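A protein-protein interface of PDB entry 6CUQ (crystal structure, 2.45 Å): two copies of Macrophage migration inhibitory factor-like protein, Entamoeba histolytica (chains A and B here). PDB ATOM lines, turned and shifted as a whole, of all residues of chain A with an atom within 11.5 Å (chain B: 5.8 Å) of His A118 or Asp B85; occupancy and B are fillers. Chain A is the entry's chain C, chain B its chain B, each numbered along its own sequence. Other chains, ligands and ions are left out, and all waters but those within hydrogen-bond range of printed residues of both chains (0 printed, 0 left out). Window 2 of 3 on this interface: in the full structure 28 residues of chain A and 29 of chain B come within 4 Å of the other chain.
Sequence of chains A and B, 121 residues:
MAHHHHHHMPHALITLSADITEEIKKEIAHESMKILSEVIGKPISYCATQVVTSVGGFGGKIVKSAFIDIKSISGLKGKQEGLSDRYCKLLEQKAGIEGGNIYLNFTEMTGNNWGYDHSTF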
ATOM      1  N   MET A   9      12.217   1.451  -3.496  1.00  0.00           N
ATOM      2  CA  MET A   9      12.210   1.887  -2.104  1.00  0.00           C
ATOM      3  C   MET A   9      10.789   2.016  -1.545  1.00  0.00           C
ATOM      4  O   MET A   9      10.400   3.086  -1.070  1.00  0.00           O
ATOM      5  CB  MET A   9      12.960   3.202  -1.935  1.00  0.00           C
ATOM      6  CG  MET A   9      14.171   3.367  -2.807  1.00  0.00           C
ATOM      7  SD  MET A   9      15.191   1.890  -2.782  1.00  0.00           S
ATOM      8  CE  MET A   9      16.255   2.268  -1.395  1.00  0.00           C
ATOM      9  N   GLY A 111      12.792  10.873  -6.947  1.00  0.00           N
ATOM     10  CA  GLY A 111      13.956  10.436  -6.198  1.00  0.00           C
ATOM     11  C   GLY A 111      14.592  11.548  -5.393  1.00  0.00           C
ATOM     12  O   GLY A 111      14.998  11.340  -4.246  1.00  0.00           O
ATOM     13  N   ASN A 112      14.683  12.746  -5.978  1.00  0.00           N
ATOM     14  CA  ASN A 112      15.297  13.864  -5.266  1.00  0.00           C
ATOM     15  C   ASN A 112      14.561  14.172  -3.963  1.00  0.00           C
ATOM     16  O   ASN A 112      15.172  14.689  -3.020  1.00  0.00           O
ATOM     17  CB  ASN A 112      15.389  15.095  -6.178  1.00  0.00           C
ATOM     18  CG  ASN A 112      14.056  15.497  -6.749  1.00  0.00           C
ATOM     19  OD1 ASN A 112      13.219  14.647  -7.043  1.00  0.00           O
ATOM     20  ND2 ASN A 112      13.846  16.801  -6.912  1.00  0.00           N
ATOM     21  N   ASN A 113      13.266  13.852  -3.881  1.00  0.00           N
ATOM     22  CA  ASN A 113      12.521  13.959  -2.633  1.00  0.00           C
ATOM     23  C   ASN A 113      12.449  12.637  -1.872  1.00  0.00           C
ATOM     24  O   ASN A 113      11.493  12.416  -1.117  1.00  0.00           O
ATOM     25  CB  ASN A 113      11.114  14.499  -2.896  1.00  0.00           C
ATOM     26  CG  ASN A 113      11.130  15.794  -3.643  1.00  0.00           C
ATOM     27  OD1 ASN A 113      11.996  16.633  -3.423  1.00  0.00           O
ATOM     28  ND2 ASN A 113      10.179  15.962  -4.551  1.00  0.00           N
ATOM     29  N   TRP A 114      13.454  11.771  -2.020  1.00  0.00           N
ATOM     30  CA  TRP A 114      13.532  10.512  -1.285  1.00  0.00           C
ATOM     31  C   TRP A 114      14.907  10.386  -0.650  1.00  0.00           C
ATOM     32  O   TRP A 114      15.915  10.272  -1.358  1.00  0.00           O
ATOM     33  CB  TRP A 114      13.273   9.295  -2.175  1.00  0.00           C
ATOM     34  CG  TRP A 114      13.031   8.102  -1.321  1.00  0.00           C
ATOM     35  CD1 TRP A 114      13.967   7.389  -0.617  1.00  0.00           C
ATOM     36  CD2 TRP A 114      11.766   7.503  -1.024  1.00  0.00           C
ATOM     37  NE1 TRP A 114      13.360   6.382   0.094  1.00  0.00           N
ATOM     38  CE2 TRP A 114      12.012   6.425  -0.142  1.00  0.00           C
ATOM     39  CE3 TRP A 114      10.452   7.765  -1.426  1.00  0.00           C
ATOM     40  CZ2 TRP A 114      10.993   5.616   0.344  1.00  0.00           C
ATOM     41  CZ3 TRP A 114       9.445   6.966  -0.940  1.00  0.00           C
ATOM     42  CH2 TRP A 114       9.719   5.899  -0.062  1.00  0.00           C
ATOM     43  N   GLY A 115      14.940  10.378   0.678  1.00  0.00           N
ATOM     44  CA  GLY A 115      16.179  10.312   1.426  1.00  0.00           C
ATOM     45  C   GLY A 115      16.425   8.938   2.017  1.00  0.00           C
ATOM     46  O   GLY A 115      15.496   8.251   2.443  1.00  0.00           O
ATOM     47  N   TYR A 116      17.704   8.559   2.062  1.00  0.00           N
ATOM     48  CA  TYR A 116      18.126   7.254   2.562  1.00  0.00           C
ATOM     49  C   TYR A 116      19.624   7.219   2.834  1.00  0.00           C
ATOM     50  O   TYR A 116      20.419   7.589   1.964  1.00  0.00           O
ATOM     51  CB  TYR A 116      17.734   6.158   1.571  1.00  0.00           C
ATOM     52  CG  TYR A 116      18.376   4.801   1.835  1.00  0.00           C
ATOM     53  CD1 TYR A 116      18.022   4.035   2.941  1.00  0.00           C
ATOM     54  CD2 TYR A 116      19.306   4.270   0.949  1.00  0.00           C
ATOM     55  CE1 TYR A 116      18.599   2.799   3.174  1.00  0.00           C
ATOM     56  CE2 TYR A 116      19.886   3.032   1.170  1.00  0.00           C
ATOM     57  CZ  TYR A 116      19.530   2.297   2.283  1.00  0.00           C
ATOM     58  OH  TYR A 116      20.110   1.057   2.498  1.00  0.00           O
ATOM     59  N   ASP A 117      20.011   6.818   4.047  1.00  0.00           N
ATOM     60  CA  ASP A 117      21.415   6.599   4.412  1.00  0.00           C
ATOM     61  C   ASP A 117      22.280   7.818   4.090  1.00  0.00           C
ATOM     62  O   ASP A 117      23.233   7.755   3.312  1.00  0.00           O
ATOM     63  CB  ASP A 117      21.965   5.346   3.716  1.00  0.00           C
ATOM     64  CG  ASP A 117      23.229   4.811   4.371  1.00  0.00           C
ATOM     65  OD1 ASP A 117      23.586   5.260   5.481  1.00  0.00           O
ATOM     66  OD2 ASP A 117      23.899   3.962   3.740  1.00  0.00           O
ATOM     67  N   HIS A 118      21.906   8.943   4.702  1.00  0.00           N
ATOM     68  CA  HIS A 118      22.600  10.231   4.674  1.00  0.00           C
ATOM     69  C   HIS A 118      22.543  10.914   3.317  1.00  0.00           C
ATOM     70  O   HIS A 118      23.128  11.991   3.167  1.00  0.00           O
ATOM     71  CB  HIS A 118      24.071  10.123   5.102  1.00  0.00           C
ATOM     72  CG  HIS A 118      24.249   9.536   6.465  1.00  0.00           C
ATOM     73  ND1 HIS A 118      24.715  10.268   7.536  1.00  0.00           N
ATOM     74  CD2 HIS A 118      24.013   8.287   6.936  1.00  0.00           C
ATOM     75  CE1 HIS A 118      24.762   9.494   8.607  1.00  0.00           C
ATOM     76  NE2 HIS A 118      24.342   8.288   8.269  1.00  0.00           N
ATOM     77  N   SER A 119      21.869  10.339   2.324  1.00  0.00           N
ATOM     78  CA  SER A 119      21.839  10.930   0.991  1.00  0.00           C
ATOM     79  C   SER A 119      20.427  10.819   0.420  1.00  0.00           C
ATOM     80  O   SER A 119      19.469  10.451   1.110  1.00  0.00           O
ATOM     81  CB  SER A 119      22.885  10.268   0.084  1.00  0.00           C
ATOM     82  OG  SER A 119      22.863  10.843  -1.210  1.00  0.00           O
ATOM     83  N   THR A 120      20.318  11.153  -0.859  1.00  0.00           N
ATOM     84  CA  THR A 120      19.082  11.190  -1.623  1.00  0.00           C
ATOM     85  C   THR A 120      19.269  10.387  -2.907  1.00  0.00           C
ATOM     86  O   THR A 120      20.361   9.891  -3.198  1.00  0.00           O
ATOM     87  CB  THR A 120      18.688  12.655  -1.902  1.00  0.00           C
ATOM     88  OG1 THR A 120      17.512  12.716  -2.723  1.00  0.00           O
ATOM     89  CG2 THR A 120      19.854  13.448  -2.543  1.00  0.00           C
ATOM     90  N   PHE A 121      18.207  10.288  -3.704  1.00  0.00           N
ATOM     91  CA  PHE A 121      18.287   9.580  -4.980  1.00  0.00           C
ATOM     92  C   PHE A 121      18.141  10.530  -6.160  1.00  0.00           C
ATOM     93  O   PHE A 121      19.136  11.051  -6.665  1.00  0.00           O
ATOM     94  CB  PHE A 121      17.228   8.477  -5.034  1.00  0.00           C
ATOM     95  CG  PHE A 121      17.584   7.265  -4.216  1.00  0.00           C
ATOM     96  CD1 PHE A 121      18.913   6.896  -4.051  1.00  0.00           C
ATOM     97  CD2 PHE A 121      16.601   6.513  -3.591  1.00  0.00           C
ATOM     98  CE1 PHE A 121      19.256   5.795  -3.298  1.00  0.00           C
ATOM     99  CE2 PHE A 121      16.938   5.407  -2.829  1.00  0.00           C
ATOM    100  CZ  PHE A 121      18.267   5.048  -2.684  1.00  0.00           C
ATOM    101  OXT PHE A 121      17.044  10.799  -6.634  1.00  0.00           O
ATOM    102  N   GLN B  80      17.619  18.764   0.207  1.00  0.00           N
ATOM    103  CA  GLN B  80      17.268  17.415   0.659  1.00  0.00           C
ATOM    104  C   GLN B  80      18.489  16.609   1.090  1.00  0.00           C
ATOM    105  O   GLN B  80      18.416  15.829   2.049  1.00  0.00           O
ATOM    106  CB  GLN B  80      16.499  16.653  -0.421  1.00  0.00           C
ATOM    107  CG  GLN B  80      15.287  17.385  -0.952  1.00  0.00           C
ATOM    108  CD  GLN B  80      15.582  18.104  -2.242  1.00  0.00           C
ATOM    109  OE1 GLN B  80      16.594  18.791  -2.362  1.00  0.00           O
ATOM    110  NE2 GLN B  80      14.687  17.969  -3.212  1.00  0.00           N
ATOM    111  N   GLU B  81      19.597  16.718   0.361  1.00  0.00           N
ATOM    112  CA  GLU B  81      20.770  15.936   0.737  1.00  0.00           C
ATOM    113  C   GLU B  81      21.281  16.334   2.120  1.00  0.00           C
ATOM    114  O   GLU B  81      21.517  15.474   2.981  1.00  0.00           O
ATOM    115  CB  GLU B  81      21.866  16.072  -0.305  1.00  0.00           C
ATOM    116  CG  GLU B  81      23.066  15.253   0.083  1.00  0.00           C
ATOM    117  CD  GLU B  81      23.803  14.692  -1.106  1.00  0.00           C
ATOM    118  OE1 GLU B  81      23.583  15.197  -2.227  1.00  0.00           O
ATOM    119  OE2 GLU B  81      24.558  13.714  -0.915  1.00  0.00           O
ATOM    120  N   GLY B  82      21.461  17.635   2.350  1.00  0.00           N
ATOM    121  CA  GLY B  82      21.923  18.081   3.653  1.00  0.00           C
ATOM    122  C   GLY B  82      20.981  17.673   4.766  1.00  0.00           C
ATOM    123  O   GLY B  82      21.413  17.312   5.865  1.00  0.00           O
ATOM    124  N   LEU B  83      19.679  17.715   4.498  1.00  0.00           N
ATOM    125  CA  LEU B  83      18.721  17.281   5.507  1.00  0.00           C
ATOM    126  C   LEU B  83      18.834  15.786   5.776  1.00  0.00           C
ATOM    127  O   LEU B  83      18.760  15.356   6.934  1.00  0.00           O
ATOM    128  CB  LEU B  83      17.310  17.656   5.078  1.00  0.00           C
ATOM    129  CG  LEU B  83      16.941  19.124   5.269  1.00  0.00           C
ATOM    130  CD1 LEU B  83      15.659  19.396   4.536  1.00  0.00           C
ATOM    131  CD2 LEU B  83      16.749  19.403   6.751  1.00  0.00           C
ATOM    132  N   SER B  84      19.018  14.975   4.730  1.00  0.00           N
ATOM    133  CA  SER B  84      19.163  13.538   4.946  1.00  0.00           C
ATOM    134  C   SER B  84      20.388  13.236   5.799  1.00  0.00           C
ATOM    135  O   SER B  84      20.332  12.392   6.704  1.00  0.00           O
ATOM    136  CB  SER B  84      19.238  12.804   3.609  1.00  0.00           C
ATOM    137  OG  SER B  84      18.174  13.200   2.767  1.00  0.00           O
ATOM    138  N   ASP B  85      21.500  13.928   5.537  1.00  0.00           N
ATOM    139  CA  ASP B  85      22.719  13.673   6.296  1.00  0.00           C
ATOM    140  C   ASP B  85      22.563  14.057   7.769  1.00  0.00           C
ATOM    141  O   ASP B  85      22.969  13.297   8.659  1.00  0.00           O
ATOM    142  CB  ASP B  85      23.891  14.421   5.654  1.00  0.00           C
ATOM    143  CG  ASP B  85      25.187  14.231   6.414  1.00  0.00           C
ATOM    144  OD1 ASP B  85      25.777  15.233   6.876  1.00  0.00           O
ATOM    145  OD2 ASP B  85      25.601  13.068   6.581  1.00  0.00           O
ATOM    146  N   ARG B  86      21.941  15.205   8.053  1.00  0.00           N
ATOM    147  CA  ARG B  86      21.844  15.660   9.439  1.00  0.00           C
ATOM    148  C   ARG B  86      20.867  14.811  10.250  1.00  0.00           C
ATOM    149  O   ARG B  86      21.122  14.518  11.424  1.00  0.00           O
ATOM    150  CB  ARG B  86      21.482  17.144   9.479  1.00  0.00           C
ATOM    151  CG  ARG B  86      22.593  18.000   8.902  1.00  0.00           C
ATOM    152  CD  ARG B  86      22.632  19.388   9.470  1.00  0.00           C
ATOM    153  NE  ARG B  86      23.005  19.403  10.878  1.00  0.00           N
ATOM    154  CZ  ARG B  86      22.821  20.451  11.674  1.00  0.00           C
ATOM    155  NH1 ARG B  86      22.266  21.549  11.187  1.00  0.00           N
ATOM    156  NH2 ARG B  86      23.175  20.396  12.950  1.00  0.00           N
ATOM    157  N   TYR B  87      19.725  14.442   9.666  1.00  0.00           N
ATOM    158  CA  TYR B  87      18.775  13.591  10.383  1.00  0.00           C
ATOM    159  C   TYR B  87      19.337  12.192  10.622  1.00  0.00           C
ATOM    160  O   TYR B  87      19.079  11.586  11.670  1.00  0.00           O
ATOM    161  CB  TYR B  87      17.457  13.499   9.619  1.00  0.00           C
ATOM    162  CG  TYR B  87      16.526  14.646   9.902  1.00  0.00           C
ATOM    163  CD1 TYR B  87      15.929  14.770  11.145  1.00  0.00           C
ATOM    164  CD2 TYR B  87      16.238  15.599   8.929  1.00  0.00           C
ATOM    165  CE1 TYR B  87      15.070  15.806  11.420  1.00  0.00           C
ATOM    166  CE2 TYR B  87      15.378  16.646   9.192  1.00  0.00           C
ATOM    167  CZ  TYR B  87      14.802  16.745  10.444  1.00  0.00           C
ATOM    168  OH  TYR B  87      13.945  17.771  10.736  1.00  0.00           O
ATOM    169  N   CYS B  88      20.052  11.638   9.638  1.00  0.00           N
ATOM    170  CA  CYS B  88      20.631  10.313   9.832  1.00  0.00           C
ATOM    171  C   CYS B  88      21.717  10.347  10.899  1.00  0.00           C
ATOM    172  O   CYS B  88      21.827   9.420  11.713  1.00  0.00           O
ATOM    173  CB  CYS B  88      21.170   9.769   8.504  1.00  0.00           C
ATOM    174  SG  CYS B  88      19.860   9.251   7.357  1.00  0.00           S
ATOM    175  N   LYS B  89      22.504  11.427  10.941  1.00  0.00           N
ATOM    176  CA  LYS B  89      23.502  11.560  11.998  1.00  0.00           C
ATOM    177  C   LYS B  89      22.832  11.739  13.350  1.00  0.00           C
ATOM    178  O   LYS B  89      23.313  11.207  14.360  1.00  0.00           O
ATOM    179  CB  LYS B  89      24.446  12.723  11.696  1.00  0.00           C
ATOM    180  N   LEU B  90      21.699  12.440  13.380  1.00  0.00           N
ATOM    181  CA  LEU B  90      20.975  12.650  14.630  1.00  0.00           C
ATOM    182  C   LEU B  90      20.393  11.346  15.183  1.00  0.00           C
ATOM    183  O   LEU B  90      20.583  11.027  16.363  1.00  0.00           O
ATOM    184  CB  LEU B  90      19.879  13.702  14.429  1.00  0.00           C
ATOM    185  CG  LEU B  90      18.989  13.808  15.668  1.00  0.00           C
ATOM    186  CD1 LEU B  90      19.871  14.228  16.817  1.00  0.00           C
ATOM    187  CD2 LEU B  90      17.774  14.742  15.499  1.00  0.00           C
ATOM    188  N   GLU B  92      21.188   8.323  14.464  1.00  0.00           N
ATOM    189  CA  GLU B  92      22.282   7.440  14.837  1.00  0.00           C
ATOM    190  C   GLU B  92      22.857   7.822  16.201  1.00  0.00           C
ATOM    191  O   GLU B  92      23.099   6.950  17.049  1.00  0.00           O
ATOM    192  CB  GLU B  92      23.359   7.466  13.753  1.00  0.00           C
ATOM    193  CG  GLU B  92      24.389   6.367  13.879  1.00  0.00           C
ATOM    194  CD  GLU B  92      25.385   6.626  14.991  1.00  0.00           C
ATOM    195  OE1 GLU B  92      25.809   7.797  15.152  1.00  0.00           O
ATOM    196  OE2 GLU B  92      25.730   5.662  15.709  1.00  0.00           O
ATOM    197  N   GLY B  99      22.047   4.324   9.190  1.00  0.00           N
ATOM    198  CA  GLY B  99      21.637   5.103   8.035  1.00  0.00           C
ATOM    199  C   GLY B  99      20.871   4.276   7.020  1.00  0.00           C
ATOM    200  O   GLY B  99      19.926   4.761   6.395  1.00  0.00           O
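Gly A115 touches Ser B84 (CA to OG, 3.8 Å).
O of Gly B99 touches CE1 of Tyr A116 (3.998 Å).
O of Glu B81 touches O of His A118 (3.8 Å).
Ser B84 touches His A118.
His A118 touches Lys B89.
Glu B81 touches Thr A120 (CB to CG2, 3.99 Å).
Of the 12 printed residues of chain A, 8 touch a printed residue of chain B.
Printed residues of chain A that touch a printed residue of chain B: Asn A112, Asn A113, Gly A115, Tyr A116, Asp A117, His A118, Ser A119 and Thr A120.
Hydrophobic or aromatic side chains of chain A that line the printed part of chain B: Tyr A116 and His A118.
Along chain A the printed residues that touch a printed residue of chain B span positions 112 to 120.
Of the 13 printed residues of chain B, 7 touch a printed residue of chain A.
Printed residues of chain B that touch a printed residue of chain A: Gln B80, Glu B81, Ser B84, Asp B85, Cys B88, Lys B89 and Gly B99.
Among the printed residues, 13 pairs touch across the chains.
Among the printed residues, no Asp or Glu carboxylate lies within 4 Å of a Lys or Arg side-chain nitrogen of the other chain.
No position is printed for both chains.
The side-chain amide nitrogen of Gln B80 lies within hydrogen-bond range of the backbone carbonyl oxygen of Asn A112, 3.3 Å away.
The side-chain amide nitrogen (NE2) of Gln B80 is in hydrogen-bond range of the side-chain amide oxygen (OD1) of Asn A113 (3.0 Å).
OG of Ser A119 is in hydrogen-bond range of OE2 of Glu B81 (3.3 Å).
O of Ser A119 lies close to OG of Ser B84 (3.5 Å).
A ring nitrogen (ND1) of His A118 sits at hydrogen-bond distance from the side-chain carboxylate of Asp B85 (3.1 Å).
The side-chain sulfur of Cys B88 lies within hydrogen-bond range of the backbone NH of His A118, 3.4 Å away.
The backbone NH (N) of Asp A117 lies close to the backbone carbonyl oxygen (O) of Gly B99 (3.1 Å).
The backbone carbonyl oxygen (O) of Gln B80 is in hydrogen-bond range of the side-chain hydroxyl (OG) of Ser B84.
O of Ser B84 is in hydrogen-bond range of SG of Cys B88.
The backbone carbonyl oxygen (O) of Gly A111 is in hydrogen-bond range of the side-chain hydroxyl (OG1) of Thr A120 (3.2 Å).
The backbone carbonyl oxygen of Asn A112 is in hydrogen-bond range of the side-chain hydroxyl of Thr A120 (3.1 Å).
OXT of Phe A121 is in hydrogen-bond range of N of Asn A112 (3.1 Å).
The backbone carbonyl oxygen (O) of Trp A114 is in hydrogen-bond range of the side-chain hydroxyl (OG1) of Thr A120, 3.2 Å away.
His A118 touches just these residues of chain B: Glu B81, Ser B84, Asp B85, Cys B88 and Lys B89.
Of chain A, only His A118 comes within 4 Å of Asp B85.
No residue of chain A comes within 4 Å of Gly B82.
Cys B88 touches one residue of chain A.
Of the printed residues of chain A, Lys B89 touches His A118 (3.8 Å).
Of the printed residues of chain B, Asp A117 touches Gly B99.
Printed residues of chain B within 4 Å of Gly A115: Ser B84.
Printed residues of chain B within 4 Å of Asn A112: Gln B80.
Printed residues of chain A within 4 Å of Gln B80: Asn A112 and Asn A113.
The nearest residue of chain A that does not touch Asp B85 is Ser A119 (4.8 Å).
The nearest printed residue of chain B that does not touch Ser A119 is Asp B85 (4.8 Å).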
